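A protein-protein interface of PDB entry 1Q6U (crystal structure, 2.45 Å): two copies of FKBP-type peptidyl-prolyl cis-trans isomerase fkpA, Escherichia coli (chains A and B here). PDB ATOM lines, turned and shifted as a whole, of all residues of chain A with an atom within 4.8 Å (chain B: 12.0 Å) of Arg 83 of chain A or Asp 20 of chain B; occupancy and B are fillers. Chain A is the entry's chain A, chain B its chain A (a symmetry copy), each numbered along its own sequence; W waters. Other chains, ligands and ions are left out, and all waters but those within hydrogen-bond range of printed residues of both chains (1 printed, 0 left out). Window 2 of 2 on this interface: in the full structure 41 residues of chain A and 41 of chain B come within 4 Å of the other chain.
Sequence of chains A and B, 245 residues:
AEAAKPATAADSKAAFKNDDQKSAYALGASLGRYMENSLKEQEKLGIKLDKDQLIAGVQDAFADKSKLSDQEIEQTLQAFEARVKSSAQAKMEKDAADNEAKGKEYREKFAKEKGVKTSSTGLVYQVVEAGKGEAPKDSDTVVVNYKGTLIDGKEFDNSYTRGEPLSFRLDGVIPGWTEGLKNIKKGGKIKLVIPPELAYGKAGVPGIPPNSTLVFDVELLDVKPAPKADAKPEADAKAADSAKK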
ATOM      1  N   ILE A  47       8.066 -14.149  13.711  1.00  0.00           N
ATOM      2  CA  ILE A  47       7.133 -13.596  14.708  1.00  0.00           C
ATOM      3  C   ILE A  47       5.768 -14.291  14.676  1.00  0.00           C
ATOM      4  O   ILE A  47       5.095 -14.291  13.656  1.00  0.00           O
ATOM      5  CB  ILE A  47       6.892 -12.118  14.441  1.00  0.00           C
ATOM      6  CG1 ILE A  47       8.087 -11.302  14.886  1.00  0.00           C
ATOM      7  CG2 ILE A  47       5.595 -11.623  15.139  1.00  0.00           C
ATOM      8  CD1 ILE A  47       8.214 -10.054  14.071  1.00  0.00           C
ATOM      9  N   LYS A  48       5.354 -14.844  15.808  1.00  0.00           N
ATOM     10  CA  LYS A  48       4.072 -15.519  15.891  1.00  0.00           C
ATOM     11  C   LYS A  48       3.161 -14.845  16.906  1.00  0.00           C
ATOM     12  O   LYS A  48       3.323 -15.045  18.103  1.00  0.00           O
ATOM     13  CB  LYS A  48       4.275 -16.982  16.254  1.00  0.00           C
ATOM     14  CG  LYS A  48       4.564 -17.853  15.052  1.00  0.00           C
ATOM     15  CD  LYS A  48       4.888 -19.315  15.439  1.00  0.00           C
ATOM     16  CE  LYS A  48       6.341 -19.497  15.917  1.00  0.00           C
ATOM     17  NZ  LYS A  48       6.740 -20.934  16.135  1.00  0.00           N
ATOM     18  N   LEU A  49       2.194 -14.064  16.420  1.00  0.00           N
ATOM     19  CA  LEU A  49       1.306 -13.325  17.306  1.00  0.00           C
ATOM     20  C   LEU A  49       0.169 -14.156  17.836  1.00  0.00           C
ATOM     21  O   LEU A  49      -0.364 -15.013  17.151  1.00  0.00           O
ATOM     22  CB  LEU A  49       0.733 -12.095  16.619  1.00  0.00           C
ATOM     23  CG  LEU A  49       1.695 -10.952  16.329  1.00  0.00           C
ATOM     24  CD1 LEU A  49       0.927  -9.786  15.681  1.00  0.00           C
ATOM     25  CD2 LEU A  49       2.362 -10.509  17.573  1.00  0.00           C
ATOM     26  N   ASP A  50      -0.204 -13.873  19.078  1.00  0.00           N
ATOM     27  CA  ASP A  50      -1.279 -14.588  19.736  1.00  0.00           C
ATOM     28  C   ASP A  50      -2.530 -14.199  18.994  1.00  0.00           C
ATOM     29  O   ASP A  50      -2.877 -13.028  18.949  1.00  0.00           O
ATOM     30  CB  ASP A  50      -1.320 -14.218  21.230  1.00  0.00           C
ATOM     31  CG  ASP A  50      -2.462 -14.907  21.995  1.00  0.00           C
ATOM     32  OD1 ASP A  50      -3.522 -15.181  21.384  1.00  0.00           O
ATOM     33  OD2 ASP A  50      -2.402 -15.189  23.218  1.00  0.00           O
ATOM     34  N   ALA A  79       6.857   0.009  18.326  1.00  0.00           N
ATOM     35  CA  ALA A  79       7.826  -0.902  18.893  1.00  0.00           C
ATOM     36  C   ALA A  79       7.778  -2.223  18.141  1.00  0.00           C
ATOM     37  O   ALA A  79       8.814  -2.856  17.945  1.00  0.00           O
ATOM     38  CB  ALA A  79       7.595  -1.105  20.375  1.00  0.00           C
ATOM     39  N   PHE A  80       6.598  -2.619  17.691  1.00  0.00           N
ATOM     40  CA  PHE A  80       6.462  -3.869  16.951  1.00  0.00           C
ATOM     41  C   PHE A  80       7.234  -3.740  15.637  1.00  0.00           C
ATOM     42  O   PHE A  80       7.874  -4.660  15.174  1.00  0.00           O
ATOM     43  CB  PHE A  80       4.976  -4.181  16.710  1.00  0.00           C
ATOM     44  CG  PHE A  80       4.725  -5.491  16.032  1.00  0.00           C
ATOM     45  CD1 PHE A  80       4.951  -6.679  16.692  1.00  0.00           C
ATOM     46  CD2 PHE A  80       4.249  -5.531  14.725  1.00  0.00           C
ATOM     47  CE1 PHE A  80       4.709  -7.908  16.048  1.00  0.00           C
ATOM     48  CE2 PHE A  80       4.011  -6.731  14.082  1.00  0.00           C
ATOM     49  CZ  PHE A  80       4.241  -7.925  14.735  1.00  0.00           C
ATOM     50  N   GLU A  81       7.213  -2.573  15.040  1.00  0.00           N
ATOM     51  CA  GLU A  81       7.946  -2.422  13.820  1.00  0.00           C
ATOM     52  C   GLU A  81       9.402  -2.714  14.083  1.00  0.00           C
ATOM     53  O   GLU A  81      10.077  -3.425  13.326  1.00  0.00           O
ATOM     54  CB  GLU A  81       7.794  -1.023  13.291  1.00  0.00           C
ATOM     55  CG  GLU A  81       6.834  -0.908  12.135  1.00  0.00           C
ATOM     56  CD  GLU A  81       6.953   0.449  11.484  1.00  0.00           C
ATOM     57  OE1 GLU A  81       7.972   0.660  10.791  1.00  0.00           O
ATOM     58  OE2 GLU A  81       6.055   1.301  11.703  1.00  0.00           O
ATOM     59  N   ALA A  82       9.895  -2.186  15.180  1.00  0.00           N
ATOM     60  CA  ALA A  82      11.286  -2.396  15.496  1.00  0.00           C
ATOM     61  C   ALA A  82      11.515  -3.869  15.733  1.00  0.00           C
ATOM     62  O   ALA A  82      12.548  -4.391  15.354  1.00  0.00           O
ATOM     63  CB  ALA A  82      11.692  -1.579  16.723  1.00  0.00           C
ATOM     64  N   ARG A  83      10.535  -4.536  16.339  1.00  0.00           N
ATOM     65  CA  ARG A  83      10.695  -5.925  16.691  1.00  0.00           C
ATOM     66  C   ARG A  83      10.650  -6.760  15.440  1.00  0.00           C
ATOM     67  O   ARG A  83      11.145  -7.853  15.405  1.00  0.00           O
ATOM     68  CB  ARG A  83       9.628  -6.381  17.672  1.00  0.00           C
ATOM     69  CG  ARG A  83       9.672  -7.883  17.985  1.00  0.00           C
ATOM     70  CD  ARG A  83       8.363  -8.478  18.485  1.00  0.00           C
ATOM     71  NE  ARG A  83       8.460  -9.859  18.973  1.00  0.00           N
ATOM     72  CZ  ARG A  83       7.413 -10.546  19.450  1.00  0.00           C
ATOM     73  NH1 ARG A  83       6.207  -9.967  19.495  1.00  0.00           N
ATOM     74  NH2 ARG A  83       7.565 -11.796  19.881  1.00  0.00           N
ATOM     75  N   VAL A  84      10.069  -6.245  14.387  1.00  0.00           N
ATOM     76  CA  VAL A  84      10.011  -7.043  13.199  1.00  0.00           C
ATOM     77  C   VAL A  84      11.338  -6.977  12.499  1.00  0.00           C
ATOM     78  O   VAL A  84      11.881  -8.023  12.137  1.00  0.00           O
ATOM     79  CB  VAL A  84       8.915  -6.600  12.273  1.00  0.00           C
ATOM     80  CG1 VAL A  84       9.028  -7.322  10.952  1.00  0.00           C
ATOM     81  CG2 VAL A  84       7.584  -6.900  12.912  1.00  0.00           C
ATOM     82  N   LYS A  85      11.844  -5.757  12.302  1.00  0.00           N
ATOM     83  CA  LYS A  85      13.135  -5.563  11.682  1.00  0.00           C
ATOM     84  C   LYS A  85      14.171  -6.394  12.431  1.00  0.00           C
ATOM     85  O   LYS A  85      15.004  -7.091  11.821  1.00  0.00           O
ATOM     86  CB  LYS A  85      13.542  -4.087  11.687  1.00  0.00           C
ATOM     87  CG  LYS A  85      12.684  -3.171  10.789  1.00  0.00           C
ATOM     88  CD  LYS A  85      13.081  -1.726  10.974  1.00  0.00           C
ATOM     89  CE  LYS A  85      12.036  -0.739  10.435  1.00  0.00           C
ATOM     90  NZ  LYS A  85      12.366  -0.187   9.082  1.00  0.00           N
ATOM     91  N   SER A  86      14.081  -6.366  13.752  1.00  0.00           N
ATOM     92  CA  SER A  86      15.044  -7.053  14.586  1.00  0.00           C
ATOM     93  C   SER A  86      14.879  -8.576  14.510  1.00  0.00           C
ATOM     94  O   SER A  86      15.867  -9.320  14.536  1.00  0.00           O
ATOM     95  CB  SER A  86      14.920  -6.548  16.030  1.00  0.00           C
ATOM     96  OG  SER A  86      15.780  -7.241  16.925  1.00  0.00           O
ATOM     97  N   SER A  87      13.644  -9.048  14.387  1.00  0.00           N
ATOM     98  CA  SER A  87      13.385 -10.492  14.389  1.00  0.00           C
ATOM     99  C   SER A  87      13.825 -11.084  13.067  1.00  0.00           C
ATOM    100  O   SER A  87      14.298 -12.200  13.011  1.00  0.00           O
ATOM    101  CB  SER A  87      11.904 -10.798  14.637  1.00  0.00           C
ATOM    102  OG  SER A  87      11.707 -12.138  15.095  1.00  0.00           O
ATOM    103  N   ALA B  15      -2.748  -6.699  31.288  1.00  0.00           N
ATOM    104  CA  ALA B  15      -3.189  -8.146  31.124  1.00  0.00           C
ATOM    105  C   ALA B  15      -2.569  -8.782  29.897  1.00  0.00           C
ATOM    106  O   ALA B  15      -3.219  -9.515  29.130  1.00  0.00           O
ATOM    107  CB  ALA B  15      -4.723  -8.273  31.048  1.00  0.00           C
ATOM    108  N   PHE B  16      -1.325  -8.436  29.675  1.00  0.00           N
ATOM    109  CA  PHE B  16      -0.570  -9.078  28.647  1.00  0.00           C
ATOM    110  C   PHE B  16       0.617  -9.647  29.340  1.00  0.00           C
ATOM    111  O   PHE B  16       1.253  -8.994  30.136  1.00  0.00           O
ATOM    112  CB  PHE B  16      -0.255  -8.043  27.572  1.00  0.00           C
ATOM    113  CG  PHE B  16      -1.470  -7.348  27.123  1.00  0.00           C
ATOM    114  CD1 PHE B  16      -2.429  -8.039  26.402  1.00  0.00           C
ATOM    115  CD2 PHE B  16      -1.741  -6.067  27.523  1.00  0.00           C
ATOM    116  CE1 PHE B  16      -3.610  -7.428  26.019  1.00  0.00           C
ATOM    117  CE2 PHE B  16      -2.917  -5.456  27.130  1.00  0.00           C
ATOM    118  CZ  PHE B  16      -3.847  -6.148  26.378  1.00  0.00           C
ATOM    119  N   LYS B  17       0.901 -10.894  29.061  1.00  0.00           N
ATOM    120  CA  LYS B  17       1.964 -11.564  29.770  1.00  0.00           C
ATOM    121  C   LYS B  17       3.262 -11.488  29.000  1.00  0.00           C
ATOM    122  O   LYS B  17       4.316 -11.805  29.524  1.00  0.00           O
ATOM    123  CB  LYS B  17       1.543 -12.989  30.015  1.00  0.00           C
ATOM    124  CG  LYS B  17       0.391 -13.014  30.963  1.00  0.00           C
ATOM    125  CD  LYS B  17       0.056 -14.407  31.409  1.00  0.00           C
ATOM    126  CE  LYS B  17      -0.921 -14.420  32.602  1.00  0.00           C
ATOM    127  NZ  LYS B  17      -2.297 -14.840  32.176  1.00  0.00           N
ATOM    128  N   ASN B  18       3.171 -11.051  27.754  1.00  0.00           N
ATOM    129  CA  ASN B  18       4.327 -10.957  26.899  1.00  0.00           C
ATOM    130  C   ASN B  18       4.028 -10.045  25.700  1.00  0.00           C
ATOM    131  O   ASN B  18       2.883  -9.650  25.490  1.00  0.00           O
ATOM    132  CB  ASN B  18       4.698 -12.354  26.422  1.00  0.00           C
ATOM    133  CG  ASN B  18       3.642 -12.956  25.460  1.00  0.00           C
ATOM    134  OD1 ASN B  18       2.876 -12.253  24.802  1.00  0.00           O
ATOM    135  ND2 ASN B  18       3.642 -14.280  25.362  1.00  0.00           N
ATOM    136  N   ASP B  19       5.067  -9.737  24.930  1.00  0.00           N
ATOM    137  CA  ASP B  19       4.978  -8.904  23.728  1.00  0.00           C
ATOM    138  C   ASP B  19       4.092  -9.520  22.651  1.00  0.00           C
ATOM    139  O   ASP B  19       3.361  -8.835  21.947  1.00  0.00           O
ATOM    140  CB  ASP B  19       6.381  -8.648  23.158  1.00  0.00           C
ATOM    141  CG  ASP B  19       7.289  -7.824  24.121  1.00  0.00           C
ATOM    142  OD1 ASP B  19       7.096  -6.586  24.178  1.00  0.00           O
ATOM    143  OD2 ASP B  19       8.216  -8.304  24.860  1.00  0.00           O
ATOM    144  N   ASP B  20       4.142 -10.830  22.528  1.00  0.00           N
ATOM    145  CA  ASP B  20       3.356 -11.476  21.505  1.00  0.00           C
ATOM    146  C   ASP B  20       1.893 -11.098  21.723  1.00  0.00           C
ATOM    147  O   ASP B  20       1.203 -10.766  20.791  1.00  0.00           O
ATOM    148  CB  ASP B  20       3.555 -13.003  21.534  1.00  0.00           C
ATOM    149  CG  ASP B  20       4.782 -13.457  20.735  1.00  0.00           C
ATOM    150  OD1 ASP B  20       5.376 -12.610  20.026  1.00  0.00           O
ATOM    151  OD2 ASP B  20       5.229 -14.654  20.752  1.00  0.00           O
ATOM    152  N   GLN B  21       1.434 -11.180  22.958  1.00  0.00           N
ATOM    153  CA  GLN B  21       0.085 -10.844  23.300  1.00  0.00           C
ATOM    154  C   GLN B  21      -0.210  -9.342  23.197  1.00  0.00           C
ATOM    155  O   GLN B  21      -1.194  -8.915  22.616  1.00  0.00           O
ATOM    156  CB  GLN B  21      -0.178 -11.344  24.703  1.00  0.00           C
ATOM    157  CG  GLN B  21      -0.163 -12.832  24.716  1.00  0.00           C
ATOM    158  CD  GLN B  21      -0.080 -13.427  26.080  1.00  0.00           C
ATOM    159  OE1 GLN B  21      -0.310 -12.751  27.068  1.00  0.00           O
ATOM    160  NE2 GLN B  21       0.266 -14.709  26.144  1.00  0.00           N
ATOM    161  N   LYS B  22       0.671  -8.530  23.714  1.00  0.00           N
ATOM    162  CA  LYS B  22       0.411  -7.106  23.702  1.00  0.00           C
ATOM    163  C   LYS B  22       0.372  -6.567  22.277  1.00  0.00           C
ATOM    164  O   LYS B  22      -0.488  -5.780  21.928  1.00  0.00           O
ATOM    165  CB  LYS B  22       1.471  -6.359  24.522  1.00  0.00           C
ATOM    166  CG  LYS B  22       0.993  -5.031  25.098  1.00  0.00           C
ATOM    167  CD  LYS B  22       2.007  -3.938  24.919  1.00  0.00           C
ATOM    168  CE  LYS B  22       1.779  -2.834  25.842  1.00  0.00           C
ATOM    169  NZ  LYS B  22       2.854  -1.875  25.661  1.00  0.00           N
ATOM    170  N   SER B  23       1.325  -6.974  21.463  1.00  0.00           N
ATOM    171  CA  SER B  23       1.367  -6.462  20.111  1.00  0.00           C
ATOM    172  C   SER B  23       0.162  -6.938  19.358  1.00  0.00           C
ATOM    173  O   SER B  23      -0.410  -6.200  18.595  1.00  0.00           O
ATOM    174  CB  SER B  23       2.605  -6.942  19.375  1.00  0.00           C
ATOM    175  OG  SER B  23       3.715  -6.432  19.992  1.00  0.00           O
ATOM    176  N   ALA B  24      -0.200  -8.190  19.546  1.00  0.00           N
ATOM    177  CA  ALA B  24      -1.323  -8.699  18.791  1.00  0.00           C
ATOM    178  C   ALA B  24      -2.566  -7.829  19.091  1.00  0.00           C
ATOM    179  O   ALA B  24      -3.294  -7.411  18.183  1.00  0.00           O
ATOM    180  CB  ALA B  24      -1.572 -10.136  19.138  1.00  0.00           C
ATOM    181  N   TYR B  25      -2.753  -7.547  20.376  1.00  0.00           N
ATOM    182  CA  TYR B  25      -3.911  -6.820  20.851  1.00  0.00           C
ATOM    183  C   TYR B  25      -3.840  -5.410  20.336  1.00  0.00           C
ATOM    184  O   TYR B  25      -4.820  -4.876  19.840  1.00  0.00           O
ATOM    185  CB  TYR B  25      -3.940  -6.862  22.373  1.00  0.00           C
ATOM    186  CG  TYR B  25      -5.135  -6.244  23.017  1.00  0.00           C
ATOM    187  CD1 TYR B  25      -5.222  -4.851  23.197  1.00  0.00           C
ATOM    188  CD2 TYR B  25      -6.166  -7.043  23.498  1.00  0.00           C
ATOM    189  CE1 TYR B  25      -6.325  -4.297  23.787  1.00  0.00           C
ATOM    190  CE2 TYR B  25      -7.293  -6.494  24.098  1.00  0.00           C
ATOM    191  CZ  TYR B  25      -7.366  -5.126  24.239  1.00  0.00           C
ATOM    192  OH  TYR B  25      -8.452  -4.581  24.855  1.00  0.00           O
ATOM    193  N   ALA B  26      -2.662  -4.825  20.394  1.00  0.00           N
ATOM    194  CA  ALA B  26      -2.537  -3.475  19.893  1.00  0.00           C
ATOM    195  C   ALA B  26      -2.922  -3.443  18.438  1.00  0.00           C
ATOM    196  O   ALA B  26      -3.585  -2.525  18.004  1.00  0.00           O
ATOM    197  CB  ALA B  26      -1.165  -2.968  20.051  1.00  0.00           C
ATOM    198  N   LEU B  27      -2.477  -4.433  17.696  1.00  0.00           N
ATOM    199  CA  LEU B  27      -2.788  -4.528  16.286  1.00  0.00           C
ATOM    200  C   LEU B  27      -4.291  -4.600  16.046  1.00  0.00           C
ATOM    201  O   LEU B  27      -4.839  -3.891  15.197  1.00  0.00           O
ATOM    202  CB  LEU B  27      -2.107  -5.735  15.648  1.00  0.00           C
ATOM    203  CG  LEU B  27      -0.645  -5.489  15.327  1.00  0.00           C
ATOM    204  CD1 LEU B  27      -0.057  -6.772  14.739  1.00  0.00           C
ATOM    205  CD2 LEU B  27      -0.503  -4.305  14.330  1.00  0.00           C
ATOM    206  N   GLY B  28      -4.963  -5.447  16.803  1.00  0.00           N
ATOM    207  CA  GLY B  28      -6.405  -5.555  16.690  1.00  0.00           C
ATOM    208  C   GLY B  28      -7.117  -4.280  17.082  1.00  0.00           C
ATOM    209  O   GLY B  28      -8.043  -3.843  16.448  1.00  0.00           O
ATOM    210  N   ALA B  29      -6.652  -3.689  18.165  1.00  0.00           N
ATOM    211  CA  ALA B  29      -7.259  -2.503  18.664  1.00  0.00           C
ATOM    212  C   ALA B  29      -7.197  -1.459  17.607  1.00  0.00           C
ATOM    213  O   ALA B  29      -8.177  -0.751  17.418  1.00  0.00           O
ATOM    214  CB  ALA B  29      -6.568  -2.021  19.922  1.00  0.00           C
ATOM    215  N   PHE B  62     -10.741 -14.854   9.348  1.00  0.00           N
ATOM    216  CA  PHE B  62      -9.572 -15.139  10.096  1.00  0.00           C
ATOM    217  C   PHE B  62      -9.484 -16.601  10.375  1.00  0.00           C
ATOM    218  O   PHE B  62      -8.391 -17.147  10.406  1.00  0.00           O
ATOM    219  CB  PHE B  62      -9.598 -14.400  11.412  1.00  0.00           C
ATOM    220  CG  PHE B  62      -8.264 -14.081  11.899  1.00  0.00           C
ATOM    221  CD1 PHE B  62      -7.485 -13.177  11.203  1.00  0.00           C
ATOM    222  CD2 PHE B  62      -7.757 -14.710  12.998  1.00  0.00           C
ATOM    223  CE1 PHE B  62      -6.225 -12.890  11.603  1.00  0.00           C
ATOM    224  CE2 PHE B  62      -6.457 -14.431  13.427  1.00  0.00           C
ATOM    225  CZ  PHE B  62      -5.698 -13.521  12.732  1.00  0.00           C
HETATM  226  O   HOH W   1       6.981 -15.237  18.350  1.00  0.00           O
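Lys 48 of chain A touches one residue of chain B. No residue of chain B comes within 4 Å of Ala 79 of chain A. Of chain B, only Ser 23 (3.5 Å) comes within 4 Å of Phe 80 of chain A. No residue of chain B comes within 4 Å of Val 84 of chain A. No residue of chain B comes within 4 Å of Ser 87 of chain A. Of the printed residues of chain A, Gln 21 of chain B touches Asp 50. Of the printed residues of chain A, Ser 23 of chain B touches Phe 80 (3.5 Å). Of the printed residues of chain A, Asp 19 of chain B touches Arg 83 (3.8 Å). Lys 17 of chain B touches none of the printed residues of chain A. The nearest printed residue of chain A that does not touch Asp 19 of chain B is Leu 49 of chain A (4.8 Å).
Of the 16 printed residues of chain B, 6 touch a printed residue of chain A. Printed residues of chain B that touch a printed residue of chain A: Asp 19, Asp 20, Gln 21, Ser 23, Ala 24 and Leu 27. Hydrophobic or aromatic side chains of chain A within 4 Å of the printed part of chain B: Leu 49 and Phe 80. Among the printed residues, 10 pairs touch across the chains.
Among the printed residues, merely in contact across the chains: Asp 50 of chain A with Ala 24 of chain B (3.2 Å), Leu 49 of chain A with Leu 27 of chain B (3.3 Å), Leu 49 of chain A with Asp 20 of chain B (3.4 Å), Phe 80 of chain A with Ser 23 of chain B (3.5 Å), Asp 50 of chain A with Gln 21 of chain B (3.6 Å), Asp 50 of chain A with Asp 20 of chain B (3.8 Å), Arg 83 of chain A with Asp 19 of chain B (3.8 Å) and Leu 49 of chain A with Ala 24 of chain B (3.9 Å).
NH1 of Arg 83 of chain A is in salt-bridge range of OD1 of Asp 20 of chain B, at 2.8 Å. The side-chain carboxylate (OD2) of Asp 20 of chain B sits close to the backbone carbonyl oxygen (O) of Lys 48 of chain A (3.3 Å).
Water W1 bridges OD2 of Asp 20 of chain B and N of Lys 48 of chain A.
The backbone NH (N) of Lys 17 of chain B lies within hydrogen-bond range of the side-chain amide oxygen (OE1) of Gln 21 of chain B. OD1 of Asn 18 of chain B is in hydrogen-bond range of N of Gln 21 of chain B, 2.6 Å away. OG of Ser 23 of chain B sits at hydrogen-bond distance from O of Asp 19 of chain B, at 3.1 Å. N of Asp 20 of chain B is in hydrogen-bond range of OD1 of Asn 18 of chain B, at 3.0 Å.
No position is printed for both chains. Of the 10 pairs that touch across the chains among the printed residues, none has its exchanged pair printed and touching as well.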
